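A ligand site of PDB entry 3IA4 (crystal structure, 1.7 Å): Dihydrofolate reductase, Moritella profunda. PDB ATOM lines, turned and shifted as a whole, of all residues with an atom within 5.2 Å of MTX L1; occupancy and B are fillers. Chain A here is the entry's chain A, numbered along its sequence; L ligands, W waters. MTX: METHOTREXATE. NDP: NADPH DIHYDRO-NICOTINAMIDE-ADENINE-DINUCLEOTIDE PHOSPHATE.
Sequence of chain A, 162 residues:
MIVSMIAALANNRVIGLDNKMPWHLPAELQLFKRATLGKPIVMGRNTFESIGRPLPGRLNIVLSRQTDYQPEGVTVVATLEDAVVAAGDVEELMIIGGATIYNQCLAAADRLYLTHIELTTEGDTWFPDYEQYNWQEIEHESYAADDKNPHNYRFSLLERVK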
ATOM      1  N   ILE A   6      22.910  17.097 -30.414  1.00  0.00           N
ATOM      2  CA  ILE A   6      22.179  18.381 -30.214  1.00  0.00           C
ATOM      3  C   ILE A   6      22.760  18.989 -28.953  1.00  0.00           C
ATOM      4  O   ILE A   6      22.896  18.304 -27.939  1.00  0.00           O
ATOM      5  CB  ILE A   6      20.640  18.210 -30.111  1.00  0.00           C
ATOM      6  CG1 ILE A   6      20.030  19.600 -29.842  1.00  0.00           C
ATOM      7  CG2 ILE A   6      20.272  17.213 -28.996  1.00  0.00           C
ATOM      8  CD1 ILE A   6      18.454  19.676 -30.085  1.00  0.00           C
ATOM      9  N   ALA A   7      23.106  20.275 -29.017  1.00  0.00           N
ATOM     10  CA  ALA A   7      23.691  20.968 -27.863  1.00  0.00           C
ATOM     11  C   ALA A   7      23.447  22.452 -27.952  1.00  0.00           C
ATOM     12  O   ALA A   7      23.288  22.966 -29.064  1.00  0.00           O
ATOM     13  CB  ALA A   7      25.248  20.752 -27.878  1.00  0.00           C
ATOM     14  N   ALA A   8      23.480  23.130 -26.799  1.00  0.00           N
ATOM     15  CA  ALA A   8      23.405  24.596 -26.795  1.00  0.00           C
ATOM     16  C   ALA A   8      24.767  25.133 -26.272  1.00  0.00           C
ATOM     17  O   ALA A   8      25.208  24.758 -25.183  1.00  0.00           O
ATOM     18  CB  ALA A   8      22.303  25.070 -25.859  1.00  0.00           C
ATOM     19  N   MET A  21      23.329  24.158 -16.624  1.00  0.00           N
ATOM     20  CA  MET A  21      23.726  25.056 -17.704  1.00  0.00           C
ATOM     21  C   MET A  21      23.717  26.452 -17.149  1.00  0.00           C
ATOM     22  O   MET A  21      22.761  26.790 -16.437  1.00  0.00           O
ATOM     23  CB  MET A  21      22.832  24.879 -18.916  1.00  0.00           C
ATOM     24  CG  MET A  21      22.987  23.433 -19.505  1.00  0.00           C
ATOM     25  SD  MET A  21      21.587  22.897 -20.482  1.00  0.00           S
ATOM     26  CE  MET A  21      21.241  24.317 -21.447  1.00  0.00           C
ATOM     27  N   GLU A  28      14.794  28.094 -24.990  1.00  0.00           N
ATOM     28  CA  GLU A  28      15.737  27.186 -25.634  1.00  0.00           C
ATOM     29  C   GLU A  28      15.348  25.733 -25.331  1.00  0.00           C
ATOM     30  O   GLU A  28      15.587  24.858 -26.158  1.00  0.00           O
ATOM     31  CB  GLU A  28      17.151  27.424 -25.151  1.00  0.00           C
ATOM     32  CG  GLU A  28      18.178  27.142 -26.231  1.00  0.00           C
ATOM     33  CD  GLU A  28      18.547  25.654 -26.378  1.00  0.00           C
ATOM     34  OE1 GLU A  28      18.651  24.980 -25.338  1.00  0.00           O
ATOM     35  OE2 GLU A  28      18.734  25.181 -27.528  1.00  0.00           O
ATOM     36  N   LEU A  29      14.739  25.477 -24.185  1.00  0.00           N
ATOM     37  CA  LEU A  29      14.325  24.074 -23.896  1.00  0.00           C
ATOM     38  C   LEU A  29      13.204  23.651 -24.789  1.00  0.00           C
ATOM     39  O   LEU A  29      13.022  22.438 -25.039  1.00  0.00           O
ATOM     40  CB  LEU A  29      13.843  23.868 -22.443  1.00  0.00           C
ATOM     41  CG  LEU A  29      14.893  24.090 -21.371  1.00  0.00           C
ATOM     42  CD1 LEU A  29      14.290  23.925 -19.928  1.00  0.00           C
ATOM     43  CD2 LEU A  29      16.079  23.145 -21.573  1.00  0.00           C
ATOM     44  N   GLN A  30      12.407  24.629 -25.227  1.00  0.00           N
ATOM     45  CA  GLN A  30      11.344  24.365 -26.192  1.00  0.00           C
ATOM     46  C   GLN A  30      11.945  24.025 -27.560  1.00  0.00           C
ATOM     47  O   GLN A  30      11.412  23.201 -28.289  1.00  0.00           O
ATOM     48  CB  GLN A  30      10.385  25.554 -26.332  1.00  0.00           C
ATOM     49  CG  GLN A  30       9.615  25.819 -25.041  1.00  0.00           C
ATOM     50  CD  GLN A  30       8.878  24.594 -24.516  1.00  0.00           C
ATOM     51  OE1 GLN A  30       8.154  23.928 -25.262  1.00  0.00           O
ATOM     52  NE2 GLN A  30       9.079  24.282 -23.233  1.00  0.00           N
ATOM     53  N   LEU A  31      13.054  24.678 -27.908  1.00  0.00           N
ATOM     54  CA  LEU A  31      13.745  24.303 -29.132  1.00  0.00           C
ATOM     55  C   LEU A  31      14.253  22.878 -29.018  1.00  0.00           C
ATOM     56  O   LEU A  31      14.160  22.088 -29.959  1.00  0.00           O
ATOM     57  CB  LEU A  31      14.930  25.287 -29.365  1.00  0.00           C
ATOM     58  CG  LEU A  31      15.786  25.160 -30.622  1.00  0.00           C
ATOM     59  CD1 LEU A  31      16.607  26.450 -30.842  1.00  0.00           C
ATOM     60  CD2 LEU A  31      16.695  23.905 -30.517  1.00  0.00           C
ATOM     61  N   PHE A  32      14.847  22.552 -27.872  1.00  0.00           N
ATOM     62  CA  PHE A  32      15.363  21.201 -27.661  1.00  0.00           C
ATOM     63  C   PHE A  32      14.215  20.177 -27.787  1.00  0.00           C
ATOM     64  O   PHE A  32      14.310  19.090 -28.409  1.00  0.00           O
ATOM     65  CB  PHE A  32      16.037  21.140 -26.282  1.00  0.00           C
ATOM     66  CG  PHE A  32      16.301  19.759 -25.779  1.00  0.00           C
ATOM     67  CD1 PHE A  32      17.458  19.056 -26.178  1.00  0.00           C
ATOM     68  CD2 PHE A  32      15.416  19.122 -24.917  1.00  0.00           C
ATOM     69  CE1 PHE A  32      17.702  17.803 -25.732  1.00  0.00           C
ATOM     70  CE2 PHE A  32      15.635  17.835 -24.500  1.00  0.00           C
ATOM     71  CZ  PHE A  32      16.805  17.174 -24.853  1.00  0.00           C
ATOM     72  N   LYS A  33      13.127  20.499 -27.134  1.00  0.00           N
ATOM     73  CA  LYS A  33      11.978  19.588 -27.208  1.00  0.00           C
ATOM     74  C   LYS A  33      11.471  19.371 -28.637  1.00  0.00           C
ATOM     75  O   LYS A  33      11.253  18.215 -29.059  1.00  0.00           O
ATOM     76  CB  LYS A  33      10.851  20.131 -26.337  1.00  0.00           C
ATOM     77  CG  LYS A  33       9.691  19.123 -26.227  1.00  0.00           C
ATOM     78  CD  LYS A  33       8.504  19.865 -25.581  1.00  0.00           C
ATOM     79  CE  LYS A  33       7.286  18.965 -25.473  1.00  0.00           C
ATOM     80  NZ  LYS A  33       7.149  18.402 -24.078  1.00  0.00           N
ATOM     81  N   THR A  36      13.835  16.998 -30.529  1.00  0.00           N
ATOM     82  CA  THR A  36      14.075  15.644 -30.034  1.00  0.00           C
ATOM     83  C   THR A  36      12.779  14.809 -29.883  1.00  0.00           C
ATOM     84  O   THR A  36      12.870  13.577 -29.809  1.00  0.00           O
ATOM     85  CB  THR A  36      14.800  15.643 -28.686  1.00  0.00           C
ATOM     86  OG1 THR A  36      14.041  16.374 -27.733  1.00  0.00           O
ATOM     87  CG2 THR A  36      16.209  16.321 -28.844  1.00  0.00           C
ATOM     88  N   THR A  47      24.396  13.993 -17.320  1.00  0.00           N
ATOM     89  CA  THR A  47      23.321  14.725 -17.996  1.00  0.00           C
ATOM     90  C   THR A  47      21.956  14.233 -17.540  1.00  0.00           C
ATOM     91  O   THR A  47      21.048  15.031 -17.245  1.00  0.00           O
ATOM     92  CB  THR A  47      23.489  14.637 -19.540  1.00  0.00           C
ATOM     93  OG1 THR A  47      24.653  15.436 -19.873  1.00  0.00           O
ATOM     94  CG2 THR A  47      22.294  15.279 -20.227  1.00  0.00           C
ATOM     95  N   SER A  50      21.253  15.700 -14.221  1.00  0.00           N
ATOM     96  CA  SER A  50      20.985  17.146 -14.384  1.00  0.00           C
ATOM     97  C   SER A  50      19.527  17.391 -14.851  1.00  0.00           C
ATOM     98  O   SER A  50      18.818  18.291 -14.356  1.00  0.00           O
ATOM     99  CB  SER A  50      21.995  17.742 -15.357  1.00  0.00           C
ATOM    100  OG  SER A  50      21.814  19.131 -15.531  1.00  0.00           O
ATOM    101  N   ILE A  51      19.044  16.589 -15.792  1.00  0.00           N
ATOM    102  CA  ILE A  51      17.657  16.730 -16.240  1.00  0.00           C
ATOM    103  C   ILE A  51      16.676  16.354 -15.120  1.00  0.00           C
ATOM    104  O   ILE A  51      15.624  17.009 -14.936  1.00  0.00           O
ATOM    105  CB  ILE A  51      17.401  15.820 -17.466  1.00  0.00           C
ATOM    106  CG1 ILE A  51      18.273  16.288 -18.613  1.00  0.00           C
ATOM    107  CG2 ILE A  51      15.907  15.912 -17.902  1.00  0.00           C
ATOM    108  CD1 ILE A  51      18.347  15.321 -19.838  1.00  0.00           C
ATOM    109  N   ARG A  53      14.648  13.697 -14.585  1.00  0.00           N
ATOM    110  CA  ARG A  53      13.538  12.793 -14.847  1.00  0.00           C
ATOM    111  C   ARG A  53      13.745  12.216 -16.230  1.00  0.00           C
ATOM    112  O   ARG A  53      14.460  12.800 -17.045  1.00  0.00           O
ATOM    113  CB  ARG A  53      12.234  13.571 -14.857  1.00  0.00           C
ATOM    114  CG  ARG A  53      12.255  14.789 -15.839  1.00  0.00           C
ATOM    115  CD  ARG A  53      10.854  15.266 -16.223  1.00  0.00           C
ATOM    116  NE  ARG A  53      10.912  16.486 -17.035  1.00  0.00           N
ATOM    117  CZ  ARG A  53       9.904  16.969 -17.760  1.00  0.00           C
ATOM    118  NH1 ARG A  53       8.720  16.359 -17.766  1.00  0.00           N
ATOM    119  NH2 ARG A  53      10.089  18.093 -18.453  1.00  0.00           N
ATOM    120  N   LEU A  55      12.501  12.112 -19.942  1.00  0.00           N
ATOM    121  CA  LEU A  55      11.725  13.022 -20.759  1.00  0.00           C
ATOM    122  C   LEU A  55      10.613  12.269 -21.529  1.00  0.00           C
ATOM    123  O   LEU A  55      10.850  11.241 -22.208  1.00  0.00           O
ATOM    124  CB  LEU A  55      12.635  13.752 -21.746  1.00  0.00           C
ATOM    125  CG  LEU A  55      13.598  14.717 -21.010  1.00  0.00           C
ATOM    126  CD1 LEU A  55      14.602  15.326 -22.011  1.00  0.00           C
ATOM    127  CD2 LEU A  55      12.771  15.803 -20.327  1.00  0.00           C
ATOM    128  N   PRO A  56       9.383  12.778 -21.474  1.00  0.00           N
ATOM    129  CA  PRO A  56       8.332  12.070 -22.238  1.00  0.00           C
ATOM    130  C   PRO A  56       8.468  12.111 -23.757  1.00  0.00           C
ATOM    131  O   PRO A  56       9.088  13.013 -24.336  1.00  0.00           O
ATOM    132  CB  PRO A  56       7.001  12.783 -21.779  1.00  0.00           C
ATOM    133  CG  PRO A  56       7.404  13.575 -20.546  1.00  0.00           C
ATOM    134  CD  PRO A  56       8.886  13.890 -20.644  1.00  0.00           C
ATOM    135  N   ARG A  58      10.006  10.317 -25.796  1.00  0.00           N
ATOM    136  CA  ARG A  58      11.337   9.890 -26.249  1.00  0.00           C
ATOM    137  C   ARG A  58      11.792   8.654 -25.545  1.00  0.00           C
ATOM    138  O   ARG A  58      11.603   8.536 -24.357  1.00  0.00           O
ATOM    139  CB  ARG A  58      12.332  11.047 -25.983  1.00  0.00           C
ATOM    140  CG  ARG A  58      12.193  12.211 -26.999  1.00  0.00           C
ATOM    141  CD  ARG A  58      12.569  13.563 -26.431  1.00  0.00           C
ATOM    142  NE  ARG A  58      11.522  13.989 -25.503  1.00  0.00           N
ATOM    143  CZ  ARG A  58      11.441  15.203 -24.974  1.00  0.00           C
ATOM    144  NH1 ARG A  58      12.361  16.175 -25.245  1.00  0.00           N
ATOM    145  NH2 ARG A  58      10.457  15.451 -24.124  1.00  0.00           N
ATOM    146  N   ILE A  96      22.399  13.789 -26.703  1.00  0.00           N
ATOM    147  CA  ILE A  96      21.961  15.062 -26.076  1.00  0.00           C
ATOM    148  C   ILE A  96      22.940  15.529 -25.031  1.00  0.00           C
ATOM    149  O   ILE A  96      22.658  16.462 -24.264  1.00  0.00           O
ATOM    150  CB  ILE A  96      20.551  15.017 -25.458  1.00  0.00           C
ATOM    151  CG1 ILE A  96      20.448  14.035 -24.259  1.00  0.00           C
ATOM    152  CG2 ILE A  96      19.551  14.596 -26.552  1.00  0.00           C
ATOM    153  CD1 ILE A  96      19.324  14.390 -23.335  1.00  0.00           C
ATOM    154  N   GLY A  97      24.060  14.830 -24.924  1.00  0.00           N
ATOM    155  CA  GLY A  97      25.139  15.279 -24.042  1.00  0.00           C
ATOM    156  C   GLY A  97      25.561  14.207 -23.035  1.00  0.00           C
ATOM    157  O   GLY A  97      24.979  13.129 -23.015  1.00  0.00           O
ATOM    158  N   TYR A 102      29.533  13.653 -26.207  1.00  0.00           N
ATOM    159  CA  TYR A 102      29.818  14.431 -27.448  1.00  0.00           C
ATOM    160  C   TYR A 102      31.251  14.146 -27.993  1.00  0.00           C
ATOM    161  O   TYR A 102      31.450  14.017 -29.195  1.00  0.00           O
ATOM    162  CB  TYR A 102      29.733  15.958 -27.212  1.00  0.00           C
ATOM    163  CG  TYR A 102      28.347  16.494 -26.882  1.00  0.00           C
ATOM    164  CD1 TYR A 102      27.223  16.090 -27.553  1.00  0.00           C
ATOM    165  CD2 TYR A 102      28.232  17.457 -25.882  1.00  0.00           C
ATOM    166  CE1 TYR A 102      25.989  16.619 -27.274  1.00  0.00           C
ATOM    167  CE2 TYR A 102      26.996  18.027 -25.562  1.00  0.00           C
ATOM    168  CZ  TYR A 102      25.889  17.621 -26.273  1.00  0.00           C
ATOM    169  OH  TYR A 102      24.713  18.193 -25.890  1.00  0.00           O
ATOM    170  N   TYR A 113      22.931  19.589 -34.248  1.00  0.00           N
ATOM    171  CA  TYR A 113      21.874  20.568 -34.070  1.00  0.00           C
ATOM    172  C   TYR A 113      22.426  21.524 -33.020  1.00  0.00           C
ATOM    173  O   TYR A 113      22.403  21.241 -31.828  1.00  0.00           O
ATOM    174  CB  TYR A 113      20.616  19.899 -33.480  1.00  0.00           C
ATOM    175  CG  TYR A 113      19.844  18.985 -34.424  1.00  0.00           C
ATOM    176  CD1 TYR A 113      18.480  19.192 -34.608  1.00  0.00           C
ATOM    177  CD2 TYR A 113      20.438  17.875 -35.041  1.00  0.00           C
ATOM    178  CE1 TYR A 113      17.740  18.354 -35.388  1.00  0.00           C
ATOM    179  CE2 TYR A 113      19.663  17.008 -35.877  1.00  0.00           C
ATOM    180  CZ  TYR A 113      18.309  17.273 -35.990  1.00  0.00           C
ATOM    181  OH  TYR A 113      17.543  16.472 -36.819  1.00  0.00           O
ATOM    182  N   THR A 115      22.567  25.133 -31.002  1.00  0.00           N
ATOM    183  CA  THR A 115      22.071  26.467 -30.668  1.00  0.00           C
ATOM    184  C   THR A 115      23.285  27.273 -30.203  1.00  0.00           C
ATOM    185  O   THR A 115      24.085  26.763 -29.411  1.00  0.00           O
ATOM    186  CB  THR A 115      21.129  26.307 -29.504  1.00  0.00           C
ATOM    187  OG1 THR A 115      19.986  25.563 -29.965  1.00  0.00           O
ATOM    188  CG2 THR A 115      20.660  27.689 -28.954  1.00  0.00           C
HETATM  189  N1  MTX L   1      19.523  22.449 -25.399  1.00  0.00           N
HETATM  190  C2  MTX L   1      20.032  21.970 -26.558  1.00  0.00           C
HETATM  191  NA2 MTX L   1      19.941  22.752 -27.639  1.00  0.00           N
HETATM  192  N3  MTX L   1      20.604  20.728 -26.612  1.00  0.00           N
HETATM  193  C4  MTX L   1      20.671  19.928 -25.503  1.00  0.00           C
HETATM  194  NA4 MTX L   1      21.255  18.758 -25.603  1.00  0.00           N
HETATM  195  C4A MTX L   1      20.122  20.385 -24.343  1.00  0.00           C
HETATM  196  N5  MTX L   1      20.137  19.570 -23.238  1.00  0.00           N
HETATM  197  C6  MTX L   1      19.606  20.041 -22.061  1.00  0.00           C
HETATM  198  C7  MTX L   1      19.018  21.297 -21.955  1.00  0.00           C
HETATM  199  N8  MTX L   1      18.976  22.115 -23.092  1.00  0.00           N
HETATM  200  C8A MTX L   1      19.538  21.636 -24.272  1.00  0.00           C
HETATM  201  C9  MTX L   1      19.682  19.123 -20.857  1.00  0.00           C
HETATM  202  N10 MTX L   1      18.855  19.566 -19.730  1.00  0.00           N
HETATM  203  CM  MTX L   1      19.566  19.982 -18.500  1.00  0.00           C
HETATM  204  C11 MTX L   1      14.651  19.525 -19.907  1.00  0.00           C
HETATM  205  C12 MTX L   1      15.296  19.988 -18.763  1.00  0.00           C
HETATM  206  C13 MTX L   1      16.678  19.988 -18.691  1.00  0.00           C
HETATM  207  C14 MTX L   1      17.418  19.555 -19.793  1.00  0.00           C
HETATM  208  C15 MTX L   1      16.744  19.123 -20.931  1.00  0.00           C
HETATM  209  C16 MTX L   1      15.385  19.027 -20.985  1.00  0.00           C
HETATM  210  C   MTX L   1      13.194  19.555 -20.064  1.00  0.00           C
HETATM  211  O   MTX L   1      12.345  19.509 -18.971  1.00  0.00           O
HETATM  212  N   MTX L   1      12.737  19.678 -21.311  1.00  0.00           N
HETATM  213  CA  MTX L   1      11.365  19.576 -21.688  1.00  0.00           C
HETATM  214  CT  MTX L   1      11.223  18.589 -22.820  1.00  0.00           C
HETATM  215  O1  MTX L   1      12.194  18.424 -23.627  1.00  0.00           O
HETATM  216  O2  MTX L   1      10.143  17.961 -22.958  1.00  0.00           O
HETATM  217  CB  MTX L   1      10.797  20.915 -22.186  1.00  0.00           C
HETATM  218  CG  MTX L   1      10.841  21.986 -21.099  1.00  0.00           C
HETATM  219  CD  MTX L   1       9.904  21.728 -19.922  1.00  0.00           C
HETATM  220  OE1 MTX L   1       9.808  22.557 -18.963  1.00  0.00           O
HETATM  221  OE2 MTX L   1       9.193  20.701 -19.863  1.00  0.00           O
HETATM  222  PA  NDP L   2      28.005  13.217 -19.198  1.00  0.00           P
HETATM  223  O1A NDP L   2      28.649  13.005 -20.549  1.00  0.00           O
HETATM  224  O2A NDP L   2      26.585  13.686 -19.074  1.00  0.00           O
HETATM  225  O5B NDP L   2      28.128  11.878 -18.261  1.00  0.00           O
HETATM  226  C5B NDP L   2      29.400  11.197 -18.189  1.00  0.00           C
HETATM  227  C4B NDP L   2      29.125   9.895 -17.458  1.00  0.00           C
HETATM  228  O4B NDP L   2      28.559   9.003 -18.415  1.00  0.00           O
HETATM  229  C3B NDP L   2      30.445   9.172 -17.085  1.00  0.00           C
HETATM  230  O3B NDP L   2      30.955   9.681 -15.857  1.00  0.00           O
HETATM  231  C2B NDP L   2      30.061   7.706 -17.059  1.00  0.00           C
HETATM  232  O2B NDP L   2      29.154   7.433 -15.983  1.00  0.00           O
HETATM  233  C1B NDP L   2      29.172   7.679 -18.281  1.00  0.00           C
HETATM  234  N9A NDP L   2      29.874   7.319 -19.529  1.00  0.00           N
HETATM  235  C8A NDP L   2      30.537   8.163 -20.331  1.00  0.00           C
HETATM  236  N7A NDP L   2      30.988   7.535 -21.428  1.00  0.00           N
HETATM  237  C5A NDP L   2      30.583   6.242 -21.342  1.00  0.00           C
HETATM  238  C6A NDP L   2      30.671   5.024 -22.158  1.00  0.00           C
HETATM  239  N6A NDP L   2      31.353   4.980 -23.353  1.00  0.00           N
HETATM  240  N1A NDP L   2      30.051   3.916 -21.637  1.00  0.00           N
HETATM  241  C2A NDP L   2      29.358   3.868 -20.497  1.00  0.00           C
HETATM  242  N3A NDP L   2      29.253   4.939 -19.722  1.00  0.00           N
HETATM  243  C4A NDP L   2      29.840   6.127 -20.106  1.00  0.00           C
HETATM  244  O3  NDP L   2      28.923  14.166 -18.273  1.00  0.00           O
HETATM  245  PN  NDP L   2      29.726  15.543 -18.438  1.00  0.00           P
HETATM  246  O1N NDP L   2      30.743  15.388 -19.502  1.00  0.00           O
HETATM  247  O2N NDP L   2      30.160  15.979 -17.083  1.00  0.00           O
HETATM  248  O5D NDP L   2      28.637  16.528 -19.042  1.00  0.00           O
HETATM  249  C5D NDP L   2      27.635  17.050 -18.181  1.00  0.00           C
HETATM  250  C4D NDP L   2      27.609  18.570 -18.306  1.00  0.00           C
HETATM  251  O4D NDP L   2      27.085  18.956 -19.622  1.00  0.00           O
HETATM  252  C3D NDP L   2      26.694  19.264 -17.275  1.00  0.00           C
HETATM  253  O3D NDP L   2      27.295  20.515 -16.901  1.00  0.00           O
HETATM  254  C2D NDP L   2      25.422  19.565 -18.068  1.00  0.00           C
HETATM  255  O2D NDP L   2      24.654  20.684 -17.544  1.00  0.00           O
HETATM  256  C1D NDP L   2      26.011  19.902 -19.410  1.00  0.00           C
HETATM  257  N1N NDP L   2      25.126  19.724 -20.551  1.00  0.00           N
HETATM  258  C2N NDP L   2      24.951  20.760 -21.367  1.00  0.00           C
HETATM  259  C3N NDP L   2      24.219  20.602 -22.521  1.00  0.00           C
HETATM  260  C7N NDP L   2      24.040  21.802 -23.406  1.00  0.00           C
HETATM  261  O7N NDP L   2      23.512  21.638 -24.490  1.00  0.00           O
HETATM  262  N7N NDP L   2      24.536  22.998 -23.088  1.00  0.00           N
HETATM  263  C4N NDP L   2      23.531  19.319 -22.942  1.00  0.00           C
HETATM  264  C5N NDP L   2      23.863  18.276 -21.993  1.00  0.00           C
HETATM  265  C6N NDP L   2      24.582  18.513 -20.842  1.00  0.00           C
HETATM  266  P2B NDP L   2      29.489   6.268 -14.893  1.00  0.00           P
HETATM  267  O1X NDP L   2      28.207   6.098 -14.217  1.00  0.00           O
HETATM  268  O2X NDP L   2      30.034   5.149 -15.721  1.00  0.00           O
HETATM  269  O3X NDP L   2      30.617   6.836 -14.075  1.00  0.00           O
HETATM  270  O   HOH W   1      11.155  25.003 -18.676  1.00  0.00           O
HETATM  271  O   HOH W   2       8.075  18.040 -21.304  1.00  0.00           O
HETATM  272  O   HOH W   3      20.237  22.864 -30.572  1.00  0.00           O
HETATM  273  O   HOH W   4       7.408  22.075 -21.790  1.00  0.00           O
HETATM  274  O   HOH W   5      13.208  18.406 -16.586  1.00  0.00           O
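A nitrogen (N3) of MTX L1 lies close to the backbone NH of Ala 7, at 3.5 Å. SD of Met 21 lies close to N8 of MTX L1 (3.8 Å). Ala 8 touches MTX L1 (N to C2, 3.6 Å). CD2 of Leu 29 touches N8 of MTX L1 (3.4 Å). Gln 30 touches MTX L1. CD1 of Phe 32 touches C4 of MTX L1, at 3.4 Å. Ser 50 touches MTX L1 (OG to CM, 3.8 Å). CG1 of Ile 51 touches N10 of MTX L1, at 3.5 Å. CD2 of Leu 55 touches C of MTX L1 (3.8 Å). OH of Tyr 102 touches NA4 of MTX L1, 3.5 Å away. Thr 115 touches MTX L1 (OG1 to NA2, 3.6 Å). Hydrophobic or aromatic side chains within 4 Å of MTX L1: Ile 6, Ala 8, Met 21, Leu 29, Phe 32, Ile 51, Leu 55 and Ile 96. 17 residues have an atom within 4 Å of MTX L1: Ile 6, Ala 7, Ala 8, Met 21, Glu 28, Leu 29, Gln 30, Phe 32, Lys 33, Ser 50, Ile 51, Arg 53, Leu 55, Arg 58, Ile 96, Tyr 102 and Thr 115. The nearest printed residue that does not touch MTX L1 is Leu 31 (4.5 Å).
The guanidinium group (NH1) of Arg 58 sits at hydrogen-bond distance from the side-chain hydroxyl (OG1) of Thr 36, 3.0 Å away. The guanidinium group (NH2) of Arg 58 lies within hydrogen-bond range of the backbone carbonyl oxygen (O) of Pro 56, 2.8 Å away. O of Ile 6 lies within hydrogen-bond range of OH of Tyr 102, at 2.7 Å. O of Ala 7 sits at hydrogen-bond distance from N of Thr 115 (3.0 Å). The backbone carbonyl oxygen (O) of Phe 32 sits at hydrogen-bond distance from the side-chain hydroxyl (OG1) of Thr 36 (2.8 Å). The backbone NH (N) of Ala 7 sits at hydrogen-bond distance from the backbone carbonyl oxygen (O) of Tyr 113 (3.1 Å). The side-chain hydroxyl (OH) of Tyr 102 lies within hydrogen-bond range of the backbone carbonyl oxygen (O) of Ile 96. The side-chain hydroxyl of Thr 115 sits at hydrogen-bond distance from the side-chain carboxylate of Glu 28 (2.8 Å).
Water W2 lies within hydrogen-bond range of an oxygen (O2) of MTX L1 (2.6 Å), the side-chain amino group (NZ) of Lys 33 (2.9 Å) and the guanidinium group (NH2) of Arg 53 (3.5 Å). Water W5 lies within hydrogen-bond range of an oxygen (O) of MTX L1, the guanidinium group of Arg 53 and the backbone carbonyl oxygen of Ile 51. Water W3 lies within hydrogen-bond range of the side-chain hydroxyl of Thr 115 (2.8 Å), a nitrogen (NA2) of MTX L1 (3.0 Å), the backbone carbonyl oxygen of Tyr 113 (3.0 Å) and the backbone carbonyl oxygen of Ala 7 (3.4 Å). Water W4 lies within hydrogen-bond range of OE2 of MTX L1 (3.0 Å) and NE2 of Gln 30 (3.1 Å).
O1 of MTX L1 is in salt-bridge range of NH1 of Arg 58 (2.8 Å). An oxygen (OE2) of MTX L1 lies within salt-bridge range of the guanidinium group (NH2) of Arg 53, 3.1 Å away. A nitrogen (N1) of MTX L1 is in hydrogen-bond range of the side-chain carboxylate of Glu 28 (2.7 Å). The side-chain amino group of Lys 33 lies within salt-bridge range of an oxygen (O2) of MTX L1. An oxygen (O2A) of NDP L2 sits at hydrogen-bond distance from the backbone NH (N) of Thr 47. An oxygen (O2A) of NDP L2 sits at hydrogen-bond distance from the side-chain hydroxyl (OG1) of Thr 47, 2.7 Å away. The backbone carbonyl oxygen of Ala 8 lies within hydrogen-bond range of a nitrogen (N7N) of NDP L2 (2.8 Å). The backbone carbonyl oxygen (O) of Ile 96 lies within hydrogen-bond range of a nitrogen (NA4) of MTX L1, 3.0 Å away. The backbone carbonyl oxygen of Ile 6 sits at hydrogen-bond distance from a nitrogen (NA4) of MTX L1, at 2.9 Å. An oxygen (O7N) of NDP L2 lies within hydrogen-bond range of the backbone NH of Ala 8 (2.7 Å).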
